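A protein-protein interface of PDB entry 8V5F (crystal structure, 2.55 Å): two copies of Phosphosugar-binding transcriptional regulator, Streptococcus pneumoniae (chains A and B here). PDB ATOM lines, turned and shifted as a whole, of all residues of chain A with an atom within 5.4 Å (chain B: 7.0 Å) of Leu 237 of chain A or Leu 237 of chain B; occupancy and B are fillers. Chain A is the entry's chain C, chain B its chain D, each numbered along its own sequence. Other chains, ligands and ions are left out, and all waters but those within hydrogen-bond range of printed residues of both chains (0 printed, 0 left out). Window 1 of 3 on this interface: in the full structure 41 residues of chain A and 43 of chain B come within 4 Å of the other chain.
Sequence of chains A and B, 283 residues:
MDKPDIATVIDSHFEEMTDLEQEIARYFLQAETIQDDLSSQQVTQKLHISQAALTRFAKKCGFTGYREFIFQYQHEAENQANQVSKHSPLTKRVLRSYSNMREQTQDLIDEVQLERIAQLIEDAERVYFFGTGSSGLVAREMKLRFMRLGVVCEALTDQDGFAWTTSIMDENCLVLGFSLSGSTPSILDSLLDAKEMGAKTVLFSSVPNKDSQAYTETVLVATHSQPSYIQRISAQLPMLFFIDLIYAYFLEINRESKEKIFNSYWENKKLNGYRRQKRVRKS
OH of Tyr 98 of chain A sits at hydrogen-bond distance from O of Leu 240 of chain B (2.9 Å).
The side-chain hydroxyl (OH) of Tyr 98 of chain A is in hydrogen-bond range of the backbone NH (N) of Phe 241 of chain B, 3.5 Å away.
The side-chain hydroxyl (OH) of Tyr 98 of chain A sits at hydrogen-bond distance from the side-chain carboxylate (OD2) of Asp 244 of chain B (2.6 Å).
The side-chain hydroxyl of Ser 234 of chain A is in hydrogen-bond range of the side-chain carboxylate of Glu 141 of chain B (3.1 Å).
N of Ser 234 of chain A lies within hydrogen-bond range of OD2 of Asp 244 of chain B.
NE2 of Gln 236 of chain A sits at hydrogen-bond distance from OE1 of Gln 236 of chain B (2.8 Å).
OH of Tyr 98 of chain B is in hydrogen-bond range of O of Leu 240 of chain A (2.7 Å).
N of Phe 241 of chain A sits at hydrogen-bond distance from OH of Tyr 98 of chain B (3.4 Å).
The backbone NH of Gln 236 of chain A lies within hydrogen-bond range of the side-chain hydroxyl of Ser 234 of chain A.
The side-chain hydroxyl of Ser 234 of chain B is in hydrogen-bond range of the backbone NH of Gln 236 of chain B.
Among the printed residues, merely in contact across the chains: Ile 233 of chain A with Asp 244 of chain B (3.1 Å), Ser 234 of chain A with Leu 240 of chain B (3.4 Å), Ala 235 of chain A with Glu 141 of chain B (3.98 Å), Gln 236 of chain A with Glu 141 of chain B (3.8 Å), Leu 237 of chain A with Leu 237 of chain B (3.8 Å) and Leu 240 of chain A with Leu 237 of chain B (3.2 Å).
Printed residues of chain B within 4 Å of Tyr 98 of chain A: Leu 240, Phe 241 and Asp 244.
Of the printed residues of chain B, Ala 235 of chain A touches Glu 141 (3.98 Å).
Of the printed residues of chain B, Phe 241 of chain A touches Tyr 98.
Thr 105 of chain B touches none of the printed residues of chain A.
His 224 of chain B touches none of the printed residues of chain A.
Of the printed residues of chain A, Gln 236 of chain B touches Gln 236.
Of the printed residues of chain A, Asp 244 of chain B touches Tyr 98 (2.6 Å), Ile 233 (3.1 Å) and Ser 234 (2.9 Å).
The nearest residue of chain A that does not touch Leu 237 of chain B is Tyr 98 of chain A (4.5 Å).
Of the 20 printed residues of chain B, 7 touch a printed residue of chain A.
Printed residues of chain B that touch a printed residue of chain A: Tyr 98, Glu 141, Gln 236, Leu 237, Leu 240, Phe 241 and Asp 244.
Of the 11 printed residues of chain A, 8 touch a printed residue of chain B.
Among the printed residues, 14 pairs touch across the chains.
Among the printed residues, no Asp or Glu carboxylate lies within 4 Å of a Lys or Arg side-chain nitrogen of the other chain.
Tyr 98 of chain A touches Leu 240 of chain B, and with the chains exchanged Leu 240 of chain A touches Tyr 98 of chain B.
Ser 234 of chain A touches Leu 240 of chain B, but with the chains exchanged Leu 240 of chain A does not touch Ser 234 of chain B (4.9 Å).
Gln 236 of chain A touches its own counterpart, Gln 236 of chain B.
Leu 240 of chain A touches Leu 237 of chain B, but with the chains exchanged Leu 237 of chain A does not touch Leu 240 of chain B (4.3 Å).
Of the 14 pairs that touch across the chains among the printed residues, 6 have their exchanged pair printed and touching as well.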
ATOM      1  N   TYR A  98       2.192  33.090  11.485  1.00  0.00           N
ATOM      2  CA  TYR A  98       2.663  32.582  10.202  1.00  0.00           C
ATOM      3  C   TYR A  98       2.050  33.360   9.042  1.00  0.00           C
ATOM      4  O   TYR A  98       2.749  33.729   8.088  1.00  0.00           O
ATOM      5  CB  TYR A  98       2.338  31.092  10.083  1.00  0.00           C
ATOM      6  CG  TYR A  98       3.383  30.160  10.686  1.00  0.00           C
ATOM      7  CD1 TYR A  98       3.583  30.085  12.069  1.00  0.00           C
ATOM      8  CD2 TYR A  98       4.172  29.359   9.868  1.00  0.00           C
ATOM      9  CE1 TYR A  98       4.537  29.232  12.610  1.00  0.00           C
ATOM     10  CE2 TYR A  98       5.125  28.507  10.396  1.00  0.00           C
ATOM     11  CZ  TYR A  98       5.305  28.446  11.766  1.00  0.00           C
ATOM     12  OH  TYR A  98       6.254  27.594  12.284  1.00  0.00           O
ATOM     13  N   MET A 101       3.649  36.738   8.828  1.00  0.00           N
ATOM     14  CA  MET A 101       4.976  36.628   8.232  1.00  0.00           C
ATOM     15  C   MET A 101       4.875  36.578   6.713  1.00  0.00           C
ATOM     16  O   MET A 101       5.631  37.258   6.011  1.00  0.00           O
ATOM     17  CB  MET A 101       5.702  35.383   8.754  1.00  0.00           C
ATOM     18  CG  MET A 101       7.213  35.388   8.496  1.00  0.00           C
ATOM     19  SD  MET A 101       8.170  34.690   9.862  1.00  0.00           S
ATOM     20  CE  MET A 101       8.347  36.121  10.936  1.00  0.00           C
ATOM     21  N   ILE A 233       7.202  32.817  17.034  1.00  0.00           N
ATOM     22  CA  ILE A 233       7.343  31.592  16.255  1.00  0.00           C
ATOM     23  C   ILE A 233       8.805  31.447  15.852  1.00  0.00           C
ATOM     24  O   ILE A 233       9.643  32.295  16.181  1.00  0.00           O
ATOM     25  CB  ILE A 233       6.423  31.596  15.020  1.00  0.00           C
ATOM     26  CG1 ILE A 233       6.721  32.799  14.112  1.00  0.00           C
ATOM     27  CG2 ILE A 233       4.972  31.596  15.456  1.00  0.00           C
ATOM     28  CD1 ILE A 233       6.601  32.494  12.633  1.00  0.00           C
ATOM     29  N   SER A 234       9.111  30.389  15.110  1.00  0.00           N
ATOM     30  CA  SER A 234      10.493  30.059  14.802  1.00  0.00           C
ATOM     31  C   SER A 234      11.235  31.245  14.208  1.00  0.00           C
ATOM     32  O   SER A 234      10.759  31.886  13.267  1.00  0.00           O
ATOM     33  CB  SER A 234      10.526  28.885  13.829  1.00  0.00           C
ATOM     34  OG  SER A 234      11.777  28.811  13.171  1.00  0.00           O
ATOM     35  N   ALA A 235      12.422  31.516  14.756  1.00  0.00           N
ATOM     36  CA  ALA A 235      13.278  32.564  14.209  1.00  0.00           C
ATOM     37  C   ALA A 235      13.802  32.211  12.823  1.00  0.00           C
ATOM     38  O   ALA A 235      14.219  33.109  12.083  1.00  0.00           O
ATOM     39  CB  ALA A 235      14.458  32.838  15.147  1.00  0.00           C
ATOM     40  N   GLN A 236      13.786  30.929  12.451  1.00  0.00           N
ATOM     41  CA  GLN A 236      14.209  30.545  11.109  1.00  0.00           C
ATOM     42  C   GLN A 236      13.337  31.212  10.045  1.00  0.00           C
ATOM     43  O   GLN A 236      13.849  31.693   9.029  1.00  0.00           O
ATOM     44  CB  GLN A 236      14.149  29.020  10.946  1.00  0.00           C
ATOM     45  CG  GLN A 236      15.415  28.248  11.309  1.00  0.00           C
ATOM     46  CD  GLN A 236      15.390  26.786  10.838  1.00  0.00           C
ATOM     47  OE1 GLN A 236      15.769  26.474   9.709  1.00  0.00           O
ATOM     48  NE2 GLN A 236      14.916  25.893  11.699  1.00  0.00           N
ATOM     49  N   LEU A 237      12.019  31.253  10.265  1.00  0.00           N
ATOM     50  CA  LEU A 237      11.052  31.419   9.179  1.00  0.00           C
ATOM     51  C   LEU A 237      11.279  32.647   8.306  1.00  0.00           C
ATOM     52  O   LEU A 237      11.187  32.524   7.073  1.00  0.00           O
ATOM     53  CB  LEU A 237       9.632  31.452   9.768  1.00  0.00           C
ATOM     54  CG  LEU A 237       8.733  30.247   9.497  1.00  0.00           C
ATOM     55  CD1 LEU A 237       8.251  30.234   8.045  1.00  0.00           C
ATOM     56  CD2 LEU A 237       9.450  28.964   9.833  1.00  0.00           C
ATOM     57  N   PRO A 238      11.553  33.831   8.847  1.00  0.00           N
ATOM     58  CA  PRO A 238      11.742  34.986   7.964  1.00  0.00           C
ATOM     59  C   PRO A 238      12.724  34.721   6.838  1.00  0.00           C
ATOM     60  O   PRO A 238      12.512  35.209   5.717  1.00  0.00           O
ATOM     61  CB  PRO A 238      12.243  36.076   8.920  1.00  0.00           C
ATOM     62  CG  PRO A 238      11.672  35.722  10.226  1.00  0.00           C
ATOM     63  CD  PRO A 238      11.549  34.211  10.271  1.00  0.00           C
ATOM     64  N   MET A 239      13.790  33.951   7.106  1.00  0.00           N
ATOM     65  CA  MET A 239      14.786  33.642   6.084  1.00  0.00           C
ATOM     66  C   MET A 239      14.339  32.504   5.176  1.00  0.00           C
ATOM     67  O   MET A 239      14.691  32.491   3.993  1.00  0.00           O
ATOM     68  CB  MET A 239      16.125  33.268   6.725  1.00  0.00           C
ATOM     69  CG  MET A 239      16.529  34.112   7.917  1.00  0.00           C
ATOM     70  SD  MET A 239      17.031  35.767   7.435  1.00  0.00           S
ATOM     71  CE  MET A 239      17.884  36.289   8.928  1.00  0.00           C
ATOM     72  N   LEU A 240      13.572  31.543   5.699  1.00  0.00           N
ATOM     73  CA  LEU A 240      13.143  30.425   4.861  1.00  0.00           C
ATOM     74  C   LEU A 240      12.313  30.924   3.691  1.00  0.00           C
ATOM     75  O   LEU A 240      12.355  30.353   2.594  1.00  0.00           O
ATOM     76  CB  LEU A 240      12.334  29.419   5.675  1.00  0.00           C
ATOM     77  CG  LEU A 240      13.084  28.435   6.567  1.00  0.00           C
ATOM     78  CD1 LEU A 240      13.839  29.228   7.606  1.00  0.00           C
ATOM     79  CD2 LEU A 240      12.186  27.429   7.267  1.00  0.00           C
ATOM     80  N   PHE A 241      11.524  31.975   3.928  1.00  0.00           N
ATOM     81  CA  PHE A 241      10.754  32.599   2.864  1.00  0.00           C
ATOM     82  C   PHE A 241      11.662  32.994   1.705  1.00  0.00           C
ATOM     83  O   PHE A 241      11.541  32.469   0.591  1.00  0.00           O
ATOM     84  CB  PHE A 241      10.003  33.815   3.423  1.00  0.00           C
ATOM     85  CG  PHE A 241       8.616  33.490   3.905  1.00  0.00           C
ATOM     86  CD1 PHE A 241       7.646  33.067   3.011  1.00  0.00           C
ATOM     87  CD2 PHE A 241       8.292  33.571   5.252  1.00  0.00           C
ATOM     88  CE1 PHE A 241       6.381  32.744   3.446  1.00  0.00           C
ATOM     89  CE2 PHE A 241       7.023  33.249   5.692  1.00  0.00           C
ATOM     90  CZ  PHE A 241       6.069  32.824   4.792  1.00  0.00           C
ATOM     91  N   TYR B  98       3.593  28.246   0.602  1.00  0.00           N
ATOM     92  CA  TYR B  98       3.708  28.575   2.015  1.00  0.00           C
ATOM     93  C   TYR B  98       2.338  28.767   2.646  1.00  0.00           C
ATOM     94  O   TYR B  98       2.158  28.470   3.833  1.00  0.00           O
ATOM     95  CB  TYR B  98       4.542  29.841   2.214  1.00  0.00           C
ATOM     96  CG  TYR B  98       6.011  29.607   2.489  1.00  0.00           C
ATOM     97  CD1 TYR B  98       6.903  29.393   1.444  1.00  0.00           C
ATOM     98  CD2 TYR B  98       6.515  29.633   3.785  1.00  0.00           C
ATOM     99  CE1 TYR B  98       8.248  29.189   1.680  1.00  0.00           C
ATOM    100  CE2 TYR B  98       7.856  29.438   4.030  1.00  0.00           C
ATOM    101  CZ  TYR B  98       8.719  29.213   2.976  1.00  0.00           C
ATOM    102  OH  TYR B  98      10.059  29.016   3.223  1.00  0.00           O
ATOM    103  N   MET B 101       0.313  25.560   2.945  1.00  0.00           N
ATOM    104  CA  MET B 101       0.823  24.801   4.081  1.00  0.00           C
ATOM    105  C   MET B 101       0.261  25.340   5.391  1.00  0.00           C
ATOM    106  O   MET B 101      -0.017  24.553   6.295  1.00  0.00           O
ATOM    107  CB  MET B 101       2.360  24.795   4.126  1.00  0.00           C
ATOM    108  CG  MET B 101       2.957  23.741   5.112  1.00  0.00           C
ATOM    109  SD  MET B 101       4.621  23.174   4.657  1.00  0.00           S
ATOM    110  CE  MET B 101       4.268  22.112   3.255  1.00  0.00           C
ATOM    111  N   THR B 105      -1.922  22.611   7.400  1.00  0.00           N
ATOM    112  CA  THR B 105      -1.587  22.481   8.812  1.00  0.00           C
ATOM    113  C   THR B 105      -2.828  22.694   9.665  1.00  0.00           C
ATOM    114  O   THR B 105      -3.171  21.861  10.509  1.00  0.00           O
ATOM    115  CB  THR B 105      -0.501  23.491   9.182  1.00  0.00           C
ATOM    116  OG1 THR B 105       0.725  23.153   8.517  1.00  0.00           O
ATOM    117  CG2 THR B 105      -0.298  23.525  10.689  1.00  0.00           C
ATOM    118  N   VAL B 138      15.247  20.514  11.929  1.00  0.00           N
ATOM    119  CA  VAL B 138      14.083  20.679  12.794  1.00  0.00           C
ATOM    120  C   VAL B 138      14.414  20.200  14.203  1.00  0.00           C
ATOM    121  O   VAL B 138      14.143  20.889  15.195  1.00  0.00           O
ATOM    122  CB  VAL B 138      12.875  19.928  12.208  1.00  0.00           C
ATOM    123  CG1 VAL B 138      11.741  19.882  13.211  1.00  0.00           C
ATOM    124  CG2 VAL B 138      12.413  20.584  10.918  1.00  0.00           C
ATOM    125  N   GLU B 141      16.506  22.707  16.009  1.00  0.00           N
ATOM    126  CA  GLU B 141      15.738  23.898  16.364  1.00  0.00           C
ATOM    127  C   GLU B 141      14.856  23.621  17.572  1.00  0.00           C
ATOM    128  O   GLU B 141      14.804  24.415  18.522  1.00  0.00           O
ATOM    129  CB  GLU B 141      14.898  24.344  15.160  1.00  0.00           C
ATOM    130  CG  GLU B 141      13.829  25.407  15.433  1.00  0.00           C
ATOM    131  CD  GLU B 141      14.366  26.829  15.411  1.00  0.00           C
ATOM    132  OE1 GLU B 141      15.594  27.007  15.257  1.00  0.00           O
ATOM    133  OE2 GLU B 141      13.553  27.775  15.519  1.00  0.00           O
ATOM    134  N   LEU B 180       9.560  13.121   7.440  1.00  0.00           N
ATOM    135  CA  LEU B 180       8.584  13.748   6.556  1.00  0.00           C
ATOM    136  C   LEU B 180       7.962  12.719   5.624  1.00  0.00           C
ATOM    137  O   LEU B 180       6.741  12.701   5.431  1.00  0.00           O
ATOM    138  CB  LEU B 180       9.248  14.867   5.756  1.00  0.00           C
ATOM    139  CG  LEU B 180       8.365  15.977   5.180  1.00  0.00           C
ATOM    140  CD1 LEU B 180       7.531  16.621   6.277  1.00  0.00           C
ATOM    141  CD2 LEU B 180       9.202  17.035   4.439  1.00  0.00           C
ATOM    142  N   VAL B 221       1.576  15.762   9.641  1.00  0.00           N
ATOM    143  CA  VAL B 221       2.071  17.077   9.261  1.00  0.00           C
ATOM    144  C   VAL B 221       1.687  17.316   7.797  1.00  0.00           C
ATOM    145  O   VAL B 221       1.219  16.415   7.102  1.00  0.00           O
ATOM    146  CB  VAL B 221       3.585  17.187   9.491  1.00  0.00           C
ATOM    147  CG1 VAL B 221       3.849  17.328  10.979  1.00  0.00           C
ATOM    148  CG2 VAL B 221       4.294  15.973   8.927  1.00  0.00           C
ATOM    149  N   ALA B 222       1.848  18.559   7.344  1.00  0.00           N
ATOM    150  CA  ALA B 222       1.359  18.952   6.029  1.00  0.00           C
ATOM    151  C   ALA B 222       2.227  18.338   4.938  1.00  0.00           C
ATOM    152  O   ALA B 222       3.454  18.291   5.059  1.00  0.00           O
ATOM    153  CB  ALA B 222       1.345  20.475   5.908  1.00  0.00           C
ATOM    154  N   HIS B 224       3.594  18.664   1.095  1.00  0.00           N
ATOM    155  CA  HIS B 224       4.007  19.827   0.314  1.00  0.00           C
ATOM    156  C   HIS B 224       3.076  19.990  -0.886  1.00  0.00           C
ATOM    157  O   HIS B 224       2.629  18.999  -1.471  1.00  0.00           O
ATOM    158  CB  HIS B 224       5.467  19.662  -0.144  1.00  0.00           C
ATOM    159  CG  HIS B 224       6.486  20.131   0.858  1.00  0.00           C
ATOM    160  ND1 HIS B 224       6.923  19.354   1.910  1.00  0.00           N
ATOM    161  CD2 HIS B 224       7.138  21.313   0.973  1.00  0.00           C
ATOM    162  CE1 HIS B 224       7.799  20.038   2.628  1.00  0.00           C
ATOM    163  NE2 HIS B 224       7.948  21.229   2.079  1.00  0.00           N
ATOM    164  N   ILE B 233       8.754  23.847  -1.614  1.00  0.00           N
ATOM    165  CA  ILE B 233       9.330  25.033  -0.979  1.00  0.00           C
ATOM    166  C   ILE B 233      10.536  24.641  -0.147  1.00  0.00           C
ATOM    167  O   ILE B 233      11.661  25.085  -0.412  1.00  0.00           O
ATOM    168  CB  ILE B 233       8.292  25.797  -0.131  1.00  0.00           C
ATOM    169  CG1 ILE B 233       7.261  24.882   0.540  1.00  0.00           C
ATOM    170  CG2 ILE B 233       7.627  26.857  -0.987  1.00  0.00           C
ATOM    171  CD1 ILE B 233       6.632  25.512   1.730  1.00  0.00           C
ATOM    172  N   SER B 234      10.330  23.765   0.828  1.00  0.00           N
ATOM    173  CA  SER B 234      11.377  23.396   1.772  1.00  0.00           C
ATOM    174  C   SER B 234      11.161  21.940   2.184  1.00  0.00           C
ATOM    175  O   SER B 234      10.577  21.153   1.432  1.00  0.00           O
ATOM    176  CB  SER B 234      11.371  24.368   2.966  1.00  0.00           C
ATOM    177  OG  SER B 234      11.929  23.737   4.107  1.00  0.00           O
ATOM    178  N   ALA B 235      11.679  21.565   3.353  1.00  0.00           N
ATOM    179  CA  ALA B 235      11.358  20.295   4.004  1.00  0.00           C
ATOM    180  C   ALA B 235      11.112  20.454   5.498  1.00  0.00           C
ATOM    181  O   ALA B 235      10.343  19.673   6.063  1.00  0.00           O
ATOM    182  CB  ALA B 235      12.475  19.262   3.779  1.00  0.00           C
ATOM    183  N   GLN B 236      11.680  21.478   6.142  1.00  0.00           N
ATOM    184  CA  GLN B 236      11.401  21.724   7.550  1.00  0.00           C
ATOM    185  C   GLN B 236       9.975  22.217   7.779  1.00  0.00           C
ATOM    186  O   GLN B 236       9.403  21.971   8.846  1.00  0.00           O
ATOM    187  CB  GLN B 236      12.358  22.777   8.110  1.00  0.00           C
ATOM    188  CG  GLN B 236      13.830  22.456   8.065  1.00  0.00           C
ATOM    189  CD  GLN B 236      14.673  23.563   8.701  1.00  0.00           C
ATOM    190  OE1 GLN B 236      14.720  23.716   9.925  1.00  0.00           O
ATOM    191  NE2 GLN B 236      15.338  24.341   7.865  1.00  0.00           N
ATOM    192  N   LEU B 237       9.391  22.922   6.811  1.00  0.00           N
ATOM    193  CA  LEU B 237       8.233  23.761   7.119  1.00  0.00           C
ATOM    194  C   LEU B 237       7.082  22.992   7.751  1.00  0.00           C
ATOM    195  O   LEU B 237       6.530  23.472   8.757  1.00  0.00           O
ATOM    196  CB  LEU B 237       7.763  24.492   5.857  1.00  0.00           C
ATOM    197  CG  LEU B 237       8.078  25.987   5.786  1.00  0.00           C
ATOM    198  CD1 LEU B 237       7.234  26.762   6.773  1.00  0.00           C
ATOM    199  CD2 LEU B 237       9.543  26.208   6.047  1.00  0.00           C
ATOM    200  N   PRO B 238       6.659  21.834   7.242  1.00  0.00           N
ATOM    201  CA  PRO B 238       5.511  21.161   7.880  1.00  0.00           C
ATOM    202  C   PRO B 238       5.710  20.943   9.377  1.00  0.00           C
ATOM    203  O   PRO B 238       4.750  21.084  10.149  1.00  0.00           O
ATOM    204  CB  PRO B 238       5.393  19.842   7.102  1.00  0.00           C
ATOM    205  CG  PRO B 238       6.030  20.130   5.746  1.00  0.00           C
ATOM    206  CD  PRO B 238       7.106  21.164   6.001  1.00  0.00           C
ATOM    207  N   MET B 239       6.939  20.643   9.810  1.00  0.00           N
ATOM    208  CA  MET B 239       7.191  20.396  11.226  1.00  0.00           C
ATOM    209  C   MET B 239       7.391  21.684  12.019  1.00  0.00           C
ATOM    210  O   MET B 239       6.951  21.770  13.174  1.00  0.00           O
ATOM    211  CB  MET B 239       8.393  19.460  11.376  1.00  0.00           C
ATOM    212  CG  MET B 239       8.094  18.030  10.933  1.00  0.00           C
ATOM    213  SD  MET B 239       9.405  17.252  10.005  1.00  0.00           S
ATOM    214  CE  MET B 239       8.620  15.675   9.685  1.00  0.00           C
ATOM    215  N   LEU B 240       8.027  22.699  11.434  1.00  0.00           N
ATOM    216  CA  LEU B 240       8.140  23.958  12.162  1.00  0.00           C
ATOM    217  C   LEU B 240       6.765  24.451  12.592  1.00  0.00           C
ATOM    218  O   LEU B 240       6.614  25.049  13.665  1.00  0.00           O
ATOM    219  CB  LEU B 240       8.829  25.028  11.321  1.00  0.00           C
ATOM    220  CG  LEU B 240      10.358  25.038  11.312  1.00  0.00           C
ATOM    221  CD1 LEU B 240      10.924  25.611  12.610  1.00  0.00           C
ATOM    222  CD2 LEU B 240      10.881  23.642  11.084  1.00  0.00           C
ATOM    223  N   PHE B 241       5.751  24.201  11.759  1.00  0.00           N
ATOM    224  CA  PHE B 241       4.387  24.599  12.099  1.00  0.00           C
ATOM    225  C   PHE B 241       3.976  24.015  13.444  1.00  0.00           C
ATOM    226  O   PHE B 241       3.543  24.744  14.345  1.00  0.00           O
ATOM    227  CB  PHE B 241       3.408  24.135  11.011  1.00  0.00           C
ATOM    228  CG  PHE B 241       3.234  25.113   9.879  1.00  0.00           C
ATOM    229  CD1 PHE B 241       2.360  26.188   9.991  1.00  0.00           C
ATOM    230  CD2 PHE B 241       3.956  24.956   8.706  1.00  0.00           C
ATOM    231  CE1 PHE B 241       2.215  27.077   8.959  1.00  0.00           C
ATOM    232  CE2 PHE B 241       3.822  25.849   7.675  1.00  0.00           C
ATOM    233  CZ  PHE B 241       2.952  26.908   7.795  1.00  0.00           C
ATOM    234  N   PHE B 242       4.122  22.693  13.595  1.00  0.00           N
ATOM    235  CA  PHE B 242       3.679  21.996  14.799  1.00  0.00           C
ATOM    236  C   PHE B 242       4.615  22.210  15.980  1.00  0.00           C
ATOM    237  O   PHE B 242       4.156  22.241  17.127  1.00  0.00           O
ATOM    238  CB  PHE B 242       3.530  20.502  14.504  1.00  0.00           C
ATOM    239  CG  PHE B 242       2.253  20.166  13.803  1.00  0.00           C
ATOM    240  CD1 PHE B 242       1.050  20.149  14.503  1.00  0.00           C
ATOM    241  CD2 PHE B 242       2.241  19.885  12.448  1.00  0.00           C
ATOM    242  CE1 PHE B 242      -0.149  19.858  13.858  1.00  0.00           C
ATOM    243  CE2 PHE B 242       1.051  19.581  11.796  1.00  0.00           C
ATOM    244  CZ  PHE B 242      -0.149  19.573  12.503  1.00  0.00           C
ATOM    245  N   ASP B 244       6.070  24.970  16.630  1.00  0.00           N
ATOM    246  CA  ASP B 244       5.655  26.267  17.136  1.00  0.00           C
ATOM    247  C   ASP B 244       4.325  26.174  17.859  1.00  0.00           C
ATOM    248  O   ASP B 244       4.079  26.939  18.796  1.00  0.00           O
ATOM    249  CB  ASP B 244       5.553  27.270  15.985  1.00  0.00           C
ATOM    250  CG  ASP B 244       6.841  28.042  15.773  1.00  0.00           C
ATOM    251  OD1 ASP B 244       7.406  28.551  16.763  1.00  0.00           O
ATOM    252  OD2 ASP B 244       7.299  28.127  14.615  1.00  0.00           O
